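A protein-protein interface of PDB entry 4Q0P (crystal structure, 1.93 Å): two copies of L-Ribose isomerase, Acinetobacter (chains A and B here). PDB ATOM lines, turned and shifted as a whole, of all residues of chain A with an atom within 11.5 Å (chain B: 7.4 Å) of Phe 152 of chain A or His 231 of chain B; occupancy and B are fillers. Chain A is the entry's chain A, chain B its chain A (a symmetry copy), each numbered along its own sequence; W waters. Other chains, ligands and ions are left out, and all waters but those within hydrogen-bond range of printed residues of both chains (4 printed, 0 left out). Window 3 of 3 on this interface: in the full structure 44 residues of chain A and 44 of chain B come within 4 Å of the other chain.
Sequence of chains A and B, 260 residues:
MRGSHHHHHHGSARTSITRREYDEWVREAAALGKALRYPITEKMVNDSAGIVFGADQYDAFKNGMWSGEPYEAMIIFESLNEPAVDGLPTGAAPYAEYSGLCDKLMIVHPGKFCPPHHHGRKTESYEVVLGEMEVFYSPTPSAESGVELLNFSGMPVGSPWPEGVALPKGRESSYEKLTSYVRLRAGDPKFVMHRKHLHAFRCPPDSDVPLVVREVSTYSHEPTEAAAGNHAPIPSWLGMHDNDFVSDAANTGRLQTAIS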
ATOM      1  N   THR A 123      -0.456  -7.193  22.758  1.00  0.00           N
ATOM      2  CA  THR A 123      -1.488  -6.809  23.715  1.00  0.00           C
ATOM      3  C   THR A 123      -2.052  -8.154  24.199  1.00  0.00           C
ATOM      4  O   THR A 123      -2.371  -9.025  23.379  1.00  0.00           O
ATOM      5  CB  THR A 123      -2.602  -5.967  23.051  1.00  0.00           C
ATOM      6  OG1 THR A 123      -2.117  -4.635  22.817  1.00  0.00           O
ATOM      7  CG2 THR A 123      -3.825  -5.897  23.944  1.00  0.00           C
ATOM      8  N   PRO A 139       0.198   1.874  34.891  1.00  0.00           N
ATOM      9  CA  PRO A 139      -0.968   2.354  34.146  1.00  0.00           C
ATOM     10  C   PRO A 139      -0.556   3.351  33.066  1.00  0.00           C
ATOM     11  O   PRO A 139      -1.361   3.733  32.217  1.00  0.00           O
ATOM     12  CB  PRO A 139      -1.828   2.990  35.231  1.00  0.00           C
ATOM     13  CG  PRO A 139      -0.795   3.563  36.153  1.00  0.00           C
ATOM     14  CD  PRO A 139       0.221   2.436  36.251  1.00  0.00           C
ATOM     15  N   PRO A 141       1.493   4.252  29.742  1.00  0.00           N
ATOM     16  CA  PRO A 141       2.093   3.534  28.613  1.00  0.00           C
ATOM     17  C   PRO A 141       3.481   4.087  28.315  1.00  0.00           C
ATOM     18  O   PRO A 141       3.757   5.256  28.582  1.00  0.00           O
ATOM     19  CB  PRO A 141       1.111   3.801  27.478  1.00  0.00           C
ATOM     20  CG  PRO A 141       0.634   5.178  27.785  1.00  0.00           C
ATOM     21  CD  PRO A 141       0.405   5.137  29.285  1.00  0.00           C
ATOM     22  N   GLU A 148       4.088   8.590  16.653  1.00  0.00           N
ATOM     23  CA  GLU A 148       2.844   8.936  17.324  1.00  0.00           C
ATOM     24  C   GLU A 148       2.112   7.622  17.547  1.00  0.00           C
ATOM     25  O   GLU A 148       2.296   6.669  16.786  1.00  0.00           O
ATOM     26  CB  GLU A 148       1.996   9.853  16.440  1.00  0.00           C
ATOM     27  CG  GLU A 148       1.426  11.062  17.166  1.00  0.00           C
ATOM     28  CD  GLU A 148      -0.062  11.246  16.924  1.00  0.00           C
ATOM     29  OE1 GLU A 148      -0.861  10.520  17.554  1.00  0.00           O
ATOM     30  OE2 GLU A 148      -0.432  12.110  16.099  1.00  0.00           O
ATOM     31  N   LEU A 149       1.282   7.569  18.583  1.00  0.00           N
ATOM     32  CA  LEU A 149       0.548   6.349  18.892  1.00  0.00           C
ATOM     33  C   LEU A 149      -0.927   6.619  19.156  1.00  0.00           C
ATOM     34  O   LEU A 149      -1.296   7.684  19.651  1.00  0.00           O
ATOM     35  CB  LEU A 149       1.178   5.664  20.108  1.00  0.00           C
ATOM     36  CG  LEU A 149       2.678   5.371  20.004  1.00  0.00           C
ATOM     37  CD1 LEU A 149       3.180   4.797  21.320  1.00  0.00           C
ATOM     38  CD2 LEU A 149       2.944   4.404  18.861  1.00  0.00           C
ATOM     39  N   LEU A 150      -1.766   5.644  18.824  1.00  0.00           N
ATOM     40  CA  LEU A 150      -3.201   5.777  19.023  1.00  0.00           C
ATOM     41  C   LEU A 150      -3.585   5.498  20.473  1.00  0.00           C
ATOM     42  O   LEU A 150      -2.874   4.798  21.195  1.00  0.00           O
ATOM     43  CB  LEU A 150      -3.954   4.820  18.094  1.00  0.00           C
ATOM     44  CG  LEU A 150      -3.715   4.984  16.587  1.00  0.00           C
ATOM     45  CD1 LEU A 150      -4.536   3.962  15.826  1.00  0.00           C
ATOM     46  CD2 LEU A 150      -4.092   6.390  16.154  1.00  0.00           C
ATOM     47  N   ASN A 151      -4.709   6.069  20.887  1.00  0.00           N
ATOM     48  CA  ASN A 151      -5.234   5.902  22.236  1.00  0.00           C
ATOM     49  C   ASN A 151      -6.733   5.688  22.121  1.00  0.00           C
ATOM     50  O   ASN A 151      -7.384   6.262  21.246  1.00  0.00           O
ATOM     51  CB  ASN A 151      -4.995   7.154  23.084  1.00  0.00           C
ATOM     52  CG  ASN A 151      -3.536   7.369  23.422  1.00  0.00           C
ATOM     53  OD1 ASN A 151      -2.927   6.571  24.136  1.00  0.00           O
ATOM     54  ND2 ASN A 151      -2.963   8.454  22.908  1.00  0.00           N
ATOM     55  N   PHE A 152      -7.276   4.849  22.994  1.00  0.00           N
ATOM     56  CA  PHE A 152      -8.706   4.598  22.999  1.00  0.00           C
ATOM     57  C   PHE A 152      -9.193   4.380  24.427  1.00  0.00           C
ATOM     58  O   PHE A 152      -9.881   5.228  24.993  1.00  0.00           O
ATOM     59  CB  PHE A 152      -9.041   3.376  22.132  1.00  0.00           C
ATOM     60  CG  PHE A 152     -10.482   2.955  22.214  1.00  0.00           C
ATOM     61  CD1 PHE A 152     -11.501   3.861  21.931  1.00  0.00           C
ATOM     62  CD2 PHE A 152     -10.821   1.659  22.590  1.00  0.00           C
ATOM     63  CE1 PHE A 152     -12.836   3.485  22.020  1.00  0.00           C
ATOM     64  CE2 PHE A 152     -12.153   1.269  22.684  1.00  0.00           C
ATOM     65  CZ  PHE A 152     -13.165   2.184  22.399  1.00  0.00           C
ATOM     66  N   SER A 153      -8.806   3.252  25.016  1.00  0.00           N
ATOM     67  CA  SER A 153      -9.226   2.921  26.370  1.00  0.00           C
ATOM     68  C   SER A 153      -8.124   3.086  27.415  1.00  0.00           C
ATOM     69  O   SER A 153      -8.403   3.408  28.570  1.00  0.00           O
ATOM     70  CB  SER A 153      -9.761   1.483  26.407  1.00  0.00           C
ATOM     71  OG  SER A 153      -8.762   0.564  25.995  1.00  0.00           O
ATOM     72  N   GLY A 154      -6.876   2.870  27.012  1.00  0.00           N
ATOM     73  CA  GLY A 154      -5.778   2.983  27.955  1.00  0.00           C
ATOM     74  C   GLY A 154      -5.956   1.937  29.041  1.00  0.00           C
ATOM     75  O   GLY A 154      -6.865   1.110  28.953  1.00  0.00           O
ATOM     76  N   MET A 155      -5.107   1.968  30.065  1.00  0.00           N
ATOM     77  CA  MET A 155      -5.195   1.004  31.163  1.00  0.00           C
ATOM     78  C   MET A 155      -5.848   1.579  32.414  1.00  0.00           C
ATOM     79  O   MET A 155      -5.658   2.751  32.737  1.00  0.00           O
ATOM     80  CB  MET A 155      -3.796   0.496  31.541  1.00  0.00           C
ATOM     81  CG  MET A 155      -3.201  -0.507  30.575  1.00  0.00           C
ATOM     82  SD  MET A 155      -4.161  -2.036  30.505  1.00  0.00           S
ATOM     83  CE  MET A 155      -3.954  -2.668  32.166  1.00  0.00           C
ATOM     84  N   PRO A 156      -6.641   0.761  33.132  1.00  0.00           N
ATOM     85  CA  PRO A 156      -7.275   1.273  34.352  1.00  0.00           C
ATOM     86  C   PRO A 156      -6.184   1.500  35.404  1.00  0.00           C
ATOM     87  O   PRO A 156      -5.141   0.846  35.373  1.00  0.00           O
ATOM     88  CB  PRO A 156      -8.249   0.156  34.738  1.00  0.00           C
ATOM     89  CG  PRO A 156      -7.601  -1.095  34.147  1.00  0.00           C
ATOM     90  CD  PRO A 156      -7.121  -0.596  32.807  1.00  0.00           C
ATOM     91  N   VAL A 192      -7.511  -6.954  30.240  1.00  0.00           N
ATOM     92  CA  VAL A 192      -6.617  -6.591  29.145  1.00  0.00           C
ATOM     93  C   VAL A 192      -5.342  -5.852  29.560  1.00  0.00           C
ATOM     94  O   VAL A 192      -5.383  -4.887  30.322  1.00  0.00           O
ATOM     95  CB  VAL A 192      -7.383  -5.718  28.102  1.00  0.00           C
ATOM     96  CG1 VAL A 192      -6.437  -5.192  27.019  1.00  0.00           C
ATOM     97  CG2 VAL A 192      -8.507  -6.533  27.488  1.00  0.00           C
ATOM     98  N   HIS A 194      -2.726  -3.834  27.733  1.00  0.00           N
ATOM     99  CA  HIS A 194      -2.345  -3.197  26.473  1.00  0.00           C
ATOM    100  C   HIS A 194      -0.844  -3.243  26.263  1.00  0.00           C
ATOM    101  O   HIS A 194      -0.073  -3.231  27.225  1.00  0.00           O
ATOM    102  CB  HIS A 194      -2.793  -1.730  26.442  1.00  0.00           C
ATOM    103  CG  HIS A 194      -4.273  -1.547  26.315  1.00  0.00           C
ATOM    104  ND1 HIS A 194      -4.987  -1.986  25.219  1.00  0.00           N
ATOM    105  CD2 HIS A 194      -5.172  -0.961  27.139  1.00  0.00           C
ATOM    106  CE1 HIS A 194      -6.262  -1.677  25.373  1.00  0.00           C
ATOM    107  NE2 HIS A 194      -6.402  -1.055  26.530  1.00  0.00           N
ATOM    108  N   ARG A 195      -0.435  -3.300  24.997  1.00  0.00           N
ATOM    109  CA  ARG A 195       0.977  -3.315  24.641  1.00  0.00           C
ATOM    110  C   ARG A 195       1.591  -2.013  25.173  1.00  0.00           C
ATOM    111  O   ARG A 195       0.871  -1.055  25.437  1.00  0.00           O
ATOM    112  CB  ARG A 195       1.131  -3.384  23.119  1.00  0.00           C
ATOM    113  CG  ARG A 195       0.395  -2.275  22.377  1.00  0.00           C
ATOM    114  CD  ARG A 195       0.677  -2.315  20.887  1.00  0.00           C
ATOM    115  NE  ARG A 195      -0.034  -3.392  20.202  1.00  0.00           N
ATOM    116  CZ  ARG A 195      -1.311  -3.327  19.835  1.00  0.00           C
ATOM    117  NH1 ARG A 195      -2.021  -2.236  20.091  1.00  0.00           N
ATOM    118  NH2 ARG A 195      -1.869  -4.346  19.193  1.00  0.00           N
ATOM    119  N   HIS A 197       3.003  -1.480  28.085  1.00  0.00           N
ATOM    120  CA  HIS A 197       2.746  -1.290  29.503  1.00  0.00           C
ATOM    121  C   HIS A 197       3.581  -2.300  30.249  1.00  0.00           C
ATOM    122  O   HIS A 197       3.576  -3.488  29.915  1.00  0.00           O
ATOM    123  CB  HIS A 197       1.276  -1.515  29.841  1.00  0.00           C
ATOM    124  CG  HIS A 197       0.405  -0.330  29.567  1.00  0.00           C
ATOM    125  ND1 HIS A 197       0.126   0.623  30.522  1.00  0.00           N
ATOM    126  CD2 HIS A 197      -0.240   0.060  28.443  1.00  0.00           C
ATOM    127  CE1 HIS A 197      -0.658   1.549  29.999  1.00  0.00           C
ATOM    128  NE2 HIS A 197      -0.895   1.231  28.738  1.00  0.00           N
ATOM    129  N   ASN B  81     -13.900  -8.558  23.251  1.00  0.00           N
ATOM    130  CA  ASN B  81     -13.901  -8.014  21.900  1.00  0.00           C
ATOM    131  C   ASN B  81     -13.135  -6.716  22.059  1.00  0.00           C
ATOM    132  O   ASN B  81     -13.698  -5.624  22.116  1.00  0.00           O
ATOM    133  CB  ASN B  81     -15.321  -7.772  21.378  1.00  0.00           C
ATOM    134  CG  ASN B  81     -15.354  -7.594  19.869  1.00  0.00           C
ATOM    135  OD1 ASN B  81     -14.494  -8.109  19.156  1.00  0.00           O
ATOM    136  ND2 ASN B  81     -16.356  -6.882  19.375  1.00  0.00           N
ATOM    137  N   GLU B  82     -11.822  -6.885  22.176  1.00  0.00           N
ATOM    138  CA  GLU B  82     -10.874  -5.810  22.383  1.00  0.00           C
ATOM    139  C   GLU B  82     -10.282  -5.268  21.080  1.00  0.00           C
ATOM    140  O   GLU B  82      -9.613  -5.989  20.342  1.00  0.00           O
ATOM    141  CB  GLU B  82      -9.757  -6.325  23.297  1.00  0.00           C
ATOM    142  CG  GLU B  82      -8.543  -5.433  23.388  1.00  0.00           C
ATOM    143  CD  GLU B  82      -8.886  -4.030  23.839  1.00  0.00           C
ATOM    144  OE1 GLU B  82      -9.708  -3.887  24.774  1.00  0.00           O
ATOM    145  OE2 GLU B  82      -8.320  -3.075  23.261  1.00  0.00           O
ATOM    146  N   PRO B  83     -10.520  -3.981  20.792  1.00  0.00           N
ATOM    147  CA  PRO B  83     -10.013  -3.326  19.581  1.00  0.00           C
ATOM    148  C   PRO B  83      -8.497  -3.451  19.440  1.00  0.00           C
ATOM    149  O   PRO B  83      -7.979  -3.623  18.336  1.00  0.00           O
ATOM    150  CB  PRO B  83     -10.444  -1.872  19.772  1.00  0.00           C
ATOM    151  CG  PRO B  83     -11.709  -1.999  20.565  1.00  0.00           C
ATOM    152  CD  PRO B  83     -11.350  -3.051  21.581  1.00  0.00           C
ATOM    153  N   ALA B  84      -7.794  -3.364  20.567  1.00  0.00           N
ATOM    154  CA  ALA B  84      -6.333  -3.440  20.589  1.00  0.00           C
ATOM    155  C   ALA B  84      -5.729  -2.283  19.790  1.00  0.00           C
ATOM    156  O   ALA B  84      -4.716  -2.446  19.099  1.00  0.00           O
ATOM    157  CB  ALA B  84      -5.856  -4.773  20.026  1.00  0.00           C
ATOM    158  N   VAL B  85      -6.362  -1.118  19.890  1.00  0.00           N
ATOM    159  CA  VAL B  85      -5.903   0.080  19.196  1.00  0.00           C
ATOM    160  C   VAL B  85      -4.837   0.823  20.004  1.00  0.00           C
ATOM    161  O   VAL B  85      -3.945   1.454  19.431  1.00  0.00           O
ATOM    162  CB  VAL B  85      -7.078   1.048  18.925  1.00  0.00           C
ATOM    163  CG1 VAL B  85      -6.551   2.384  18.420  1.00  0.00           C
ATOM    164  CG2 VAL B  85      -8.029   0.437  17.900  1.00  0.00           C
ATOM    165  N   ASP B  86      -4.927   0.748  21.331  1.00  0.00           N
ATOM    166  CA  ASP B  86      -3.962   1.423  22.196  1.00  0.00           C
ATOM    167  C   ASP B  86      -2.531   0.937  21.967  1.00  0.00           C
ATOM    168  O   ASP B  86      -2.270  -0.268  21.966  1.00  0.00           O
ATOM    169  CB  ASP B  86      -4.330   1.227  23.678  1.00  0.00           C
ATOM    170  CG  ASP B  86      -5.616   1.946  24.066  1.00  0.00           C
ATOM    171  OD1 ASP B  86      -6.716   1.481  23.696  1.00  0.00           O
ATOM    172  OD2 ASP B  86      -5.522   2.991  24.745  1.00  0.00           O
ATOM    173  N   GLY B  87      -1.608   1.878  21.773  1.00  0.00           N
ATOM    174  CA  GLY B  87      -0.214   1.524  21.570  1.00  0.00           C
ATOM    175  C   GLY B  87       0.202   1.350  20.123  1.00  0.00           C
ATOM    176  O   GLY B  87       1.382   1.145  19.826  1.00  0.00           O
ATOM    177  N   TYR B 219     -10.799  -8.867  16.125  1.00  0.00           N
ATOM    178  CA  TYR B 219     -11.990  -8.080  16.431  1.00  0.00           C
ATOM    179  C   TYR B 219     -13.206  -8.448  15.590  1.00  0.00           C
ATOM    180  O   TYR B 219     -13.094  -8.699  14.394  1.00  0.00           O
ATOM    181  CB  TYR B 219     -11.692  -6.589  16.260  1.00  0.00           C
ATOM    182  CG  TYR B 219     -12.722  -5.683  16.892  1.00  0.00           C
ATOM    183  CD1 TYR B 219     -12.691  -5.409  18.263  1.00  0.00           C
ATOM    184  CD2 TYR B 219     -13.721  -5.085  16.125  1.00  0.00           C
ATOM    185  CE1 TYR B 219     -13.627  -4.559  18.853  1.00  0.00           C
ATOM    186  CE2 TYR B 219     -14.664  -4.230  16.706  1.00  0.00           C
ATOM    187  CZ  TYR B 219     -14.607  -3.973  18.070  1.00  0.00           C
ATOM    188  OH  TYR B 219     -15.520  -3.121  18.646  1.00  0.00           O
ATOM    189  N   ALA B 227     -24.966  -3.776  20.577  1.00  0.00           N
ATOM    190  CA  ALA B 227     -23.728  -3.094  20.216  1.00  0.00           C
ATOM    191  C   ALA B 227     -23.961  -1.593  20.054  1.00  0.00           C
ATOM    192  O   ALA B 227     -23.170  -0.778  20.531  1.00  0.00           O
ATOM    193  CB  ALA B 227     -23.168  -3.679  18.920  1.00  0.00           C
ATOM    194  N   GLY B 229     -24.344   1.707  20.692  1.00  0.00           N
ATOM    195  CA  GLY B 229     -24.257   2.515  21.897  1.00  0.00           C
ATOM    196  C   GLY B 229     -22.833   2.758  22.375  1.00  0.00           C
ATOM    197  O   GLY B 229     -22.579   3.684  23.146  1.00  0.00           O
ATOM    198  N   ASN B 230     -21.903   1.927  21.910  1.00  0.00           N
ATOM    199  CA  ASN B 230     -20.495   2.042  22.289  1.00  0.00           C
ATOM    200  C   ASN B 230     -19.770   3.137  21.508  1.00  0.00           C
ATOM    201  O   ASN B 230     -20.308   3.695  20.551  1.00  0.00           O
ATOM    202  CB  ASN B 230     -19.778   0.704  22.065  1.00  0.00           C
ATOM    203  CG  ASN B 230     -20.402  -0.435  22.847  1.00  0.00           C
ATOM    204  OD1 ASN B 230     -20.486  -0.387  24.075  1.00  0.00           O
ATOM    205  ND2 ASN B 230     -20.840  -1.472  22.139  1.00  0.00           N
ATOM    206  N   HIS B 231     -18.548   3.441  21.935  1.00  0.00           N
ATOM    207  CA  HIS B 231     -17.717   4.455  21.288  1.00  0.00           C
ATOM    208  C   HIS B 231     -16.780   3.761  20.298  1.00  0.00           C
ATOM    209  O   HIS B 231     -16.267   2.678  20.580  1.00  0.00           O
ATOM    210  CB  HIS B 231     -16.899   5.201  22.349  1.00  0.00           C
ATOM    211  CG  HIS B 231     -15.977   6.244  21.794  1.00  0.00           C
ATOM    212  ND1 HIS B 231     -15.028   6.881  22.567  1.00  0.00           N
ATOM    213  CD2 HIS B 231     -15.858   6.765  20.550  1.00  0.00           C
ATOM    214  CE1 HIS B 231     -14.365   7.748  21.822  1.00  0.00           C
ATOM    215  NE2 HIS B 231     -14.849   7.697  20.594  1.00  0.00           N
ATOM    216  N   ALA B 232     -16.565   4.381  19.140  1.00  0.00           N
ATOM    217  CA  ALA B 232     -15.690   3.809  18.120  1.00  0.00           C
ATOM    218  C   ALA B 232     -14.230   4.196  18.350  1.00  0.00           C
ATOM    219  O   ALA B 232     -13.901   5.379  18.459  1.00  0.00           O
ATOM    220  CB  ALA B 232     -16.138   4.262  16.734  1.00  0.00           C
ATOM    221  N   PRO B 233     -13.332   3.198  18.424  1.00  0.00           N
ATOM    222  CA  PRO B 233     -11.900   3.433  18.642  1.00  0.00           C
ATOM    223  C   PRO B 233     -11.250   4.179  17.480  1.00  0.00           C
ATOM    224  O   PRO B 233     -10.347   4.992  17.671  1.00  0.00           O
ATOM    225  CB  PRO B 233     -11.348   2.021  18.815  1.00  0.00           C
ATOM    226  CG  PRO B 233     -12.242   1.210  17.942  1.00  0.00           C
ATOM    227  CD  PRO B 233     -13.607   1.759  18.270  1.00  0.00           C
ATOM    228  N   ILE B 234     -11.717   3.883  16.272  1.00  0.00           N
ATOM    229  CA  ILE B 234     -11.223   4.522  15.060  1.00  0.00           C
ATOM    230  C   ILE B 234     -12.458   4.871  14.237  1.00  0.00           C
ATOM    231  O   ILE B 234     -13.371   4.057  14.101  1.00  0.00           O
ATOM    232  CB  ILE B 234     -10.292   3.579  14.261  1.00  0.00           C
ATOM    233  CG1 ILE B 234      -9.005   3.337  15.056  1.00  0.00           C
ATOM    234  CG2 ILE B 234      -9.967   4.181  12.905  1.00  0.00           C
ATOM    235  CD1 ILE B 234      -8.026   2.395  14.388  1.00  0.00           C
ATOM    236  N   TRP B 237     -14.301   2.367  11.808  1.00  0.00           N
ATOM    237  CA  TRP B 237     -14.967   1.261  12.491  1.00  0.00           C
ATOM    238  C   TRP B 237     -16.459   1.476  12.733  1.00  0.00           C
ATOM    239  O   TRP B 237     -17.226   0.517  12.765  1.00  0.00           O
ATOM    240  CB  TRP B 237     -14.276   0.991  13.829  1.00  0.00           C
ATOM    241  CG  TRP B 237     -12.877   0.461  13.706  1.00  0.00           C
ATOM    242  CD1 TRP B 237     -11.950   0.797  12.761  1.00  0.00           C
ATOM    243  CD2 TRP B 237     -12.230  -0.455  14.595  1.00  0.00           C
ATOM    244  NE1 TRP B 237     -10.764   0.150  13.009  1.00  0.00           N
ATOM    245  CE2 TRP B 237     -10.908  -0.623  14.132  1.00  0.00           C
ATOM    246  CE3 TRP B 237     -12.638  -1.145  15.745  1.00  0.00           C
ATOM    247  CZ2 TRP B 237      -9.988  -1.457  14.776  1.00  0.00           C
ATOM    248  CZ3 TRP B 237     -11.723  -1.973  16.386  1.00  0.00           C
ATOM    249  CH2 TRP B 237     -10.412  -2.120  15.899  1.00  0.00           C
ATOM    250  N   LEU B 238     -16.870   2.728  12.909  1.00  0.00           N
ATOM    251  CA  LEU B 238     -18.278   3.026  13.160  1.00  0.00           C
ATOM    252  C   LEU B 238     -19.186   2.446  12.076  1.00  0.00           C
ATOM    253  O   LEU B 238     -19.003   2.717  10.889  1.00  0.00           O
ATOM    254  CB  LEU B 238     -18.497   4.541  13.253  1.00  0.00           C
ATOM    255  CG  LEU B 238     -19.917   4.986  13.622  1.00  0.00           C
ATOM    256  CD1 LEU B 238     -20.275   4.477  15.011  1.00  0.00           C
ATOM    257  CD2 LEU B 238     -20.003   6.503  13.577  1.00  0.00           C
HETATM  258  O   HOH W   1      -3.804  -2.541  22.756  1.00  0.00           O
HETATM  259  O   HOH W   2      -0.388   1.431  24.873  1.00  0.00           O
HETATM  260  O   HOH W   3      -3.251   4.279  25.864  1.00  0.00           O
HETATM  261  O   HOH W   4      -3.353  -4.272  16.815  1.00  0.00           O
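O of Leu 150 of chain A sits at hydrogen-bond distance from N of Gly 87 of chain B (3.2 Å).
The backbone NH (N) of Phe 152 of chain A is in hydrogen-bond range of the side-chain carboxylate (OD2) of Asp 86 of chain B, at 3.1 Å.
The backbone NH of Ser 153 of chain A lies within hydrogen-bond range of the side-chain carboxylate of Asp 86 of chain B, 3.0 Å away.
The backbone NH (N) of Gly 154 of chain A lies within hydrogen-bond range of the side-chain carboxylate (OD2) of Asp 86 of chain B (2.6 Å).
The guanidinium group (NH1) of Arg 195 of chain A lies within hydrogen-bond range of the backbone carbonyl oxygen (O) of Ala 84 of chain B (2.9 Å).
NH1 of Arg 195 of chain A is in hydrogen-bond range of O of Asp 86 of chain B, 2.7 Å away.
The side-chain hydroxyl of Thr 123 of chain A is in hydrogen-bond range of the backbone NH of Arg 195 of chain A, 3.1 Å away.
The side-chain hydroxyl (OG) of Ser 153 of chain A sits at hydrogen-bond distance from a ring nitrogen (NE2) of His 194 of chain A, at 2.9 Å.
The backbone carbonyl oxygen of Gly 154 of chain A lies close to a ring nitrogen (NE2) of His 194 of chain A.
The backbone NH of His 194 of chain A lies within hydrogen-bond range of the side-chain sulfur of Met 155 of chain A (3.6 Å).
The side-chain carboxylate (OE2) of Glu 82 of chain B is in hydrogen-bond range of the backbone NH (N) of Ala 84 of chain B (2.8 Å).
CD2 of Leu 149 of chain A touches O of Gly 87 of chain B, at 3.7 Å.
Leu 150 of chain A touches Val 85 of chain B.
O of Leu 150 of chain A touches CA of Asp 86 of chain B, 3.7 Å away.
CA of Asn 151 of chain A touches OD2 of Asp 86 of chain B (3.9 Å).
Phe 152 of chain A touches Pro 83 of chain B.
CZ of Phe 152 of chain A touches O of His 231 of chain B (3.6 Å).
CE1 of Phe 152 of chain A touches C of Ala 232 of chain B, 3.99 Å away.
Glu 82 of chain B touches Val 192 of chain A.
His 194 of chain A touches Glu 82 of chain B.
Asp 86 of chain B touches His 194 of chain A (OD1 to CE1, 3.6 Å).
Of the printed residues of chain B, Phe 152 of chain A touches Pro 83 (3.9 Å), Asp 86 (3.1 Å), His 231 (3.6 Å), Ala 232 (3.99 Å) and Pro 233 (3.3 Å).
Of chain A, only Phe 152 (3.6 Å) comes within 4 Å of His 231 of chain B.
Of chain A, only Phe 152 (3.9 Å) comes within 4 Å of Pro 83 of chain B.
No residue of chain A comes within 4 Å of Asn 230 of chain B.
Of the printed residues of chain B, Ser 153 of chain A touches Asp 86.
Of the printed residues of chain B, Arg 195 of chain A touches Ala 84 (2.9 Å), Asp 86 (2.7 Å) and Gly 87 (3.7 Å).
Of the printed residues of chain B, Asn 151 of chain A touches Asp 86.
Printed residues of chain B within 4 Å of His 194 of chain A: Glu 82 and Asp 86.
Of the printed residues of chain B, Val 192 of chain A touches Glu 82 (3.98 Å).
Met 155 of chain A touches none of the printed residues of chain B.
The nearest printed residue of chain B that does not touch Phe 152 of chain A is Val 85 of chain B (4.4 Å).
The nearest residue of chain A that does not touch His 231 of chain B is Asn 151 of chain A (7.2 Å).
Of the 16 printed residues of chain A, 9 touch a printed residue of chain B.
Hydrophobic or aromatic side chains of chain A that line the printed part of chain B: Leu 149, Leu 150, Phe 152, Val 192 and His 194.
Along chain A the printed residues that touch a printed residue of chain B span positions 149 to 195.
Among the printed residues, no Asp or Glu carboxylate lies within 4 Å of a Lys or Arg side-chain nitrogen of the other chain.
No position is printed for both chains.
Water W1 lies within hydrogen-bond range of OG1 of Thr 123 of chain A (2.7 Å), ND1 of His 194 of chain A (2.8 Å), O of Asp 86 of chain B (2.9 Å) and NH1 of Arg 195 of chain A (3.2 Å).
Water W4 bridges NH2 of Arg 195 of chain A (2.8 Å) and O of Ala 84 of chain B (3.2 Å).
Water W3 lies within hydrogen-bond range of the side-chain carboxylate of Asp 86 of chain B (2.8 Å) and the side-chain amide oxygen of Asn 151 of chain A (2.9 Å).
Water W2 bridges the backbone carbonyl oxygen of Arg 195 of chain A (2.8 Å) and the backbone NH of Gly 87 of chain B (3.4 Å).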
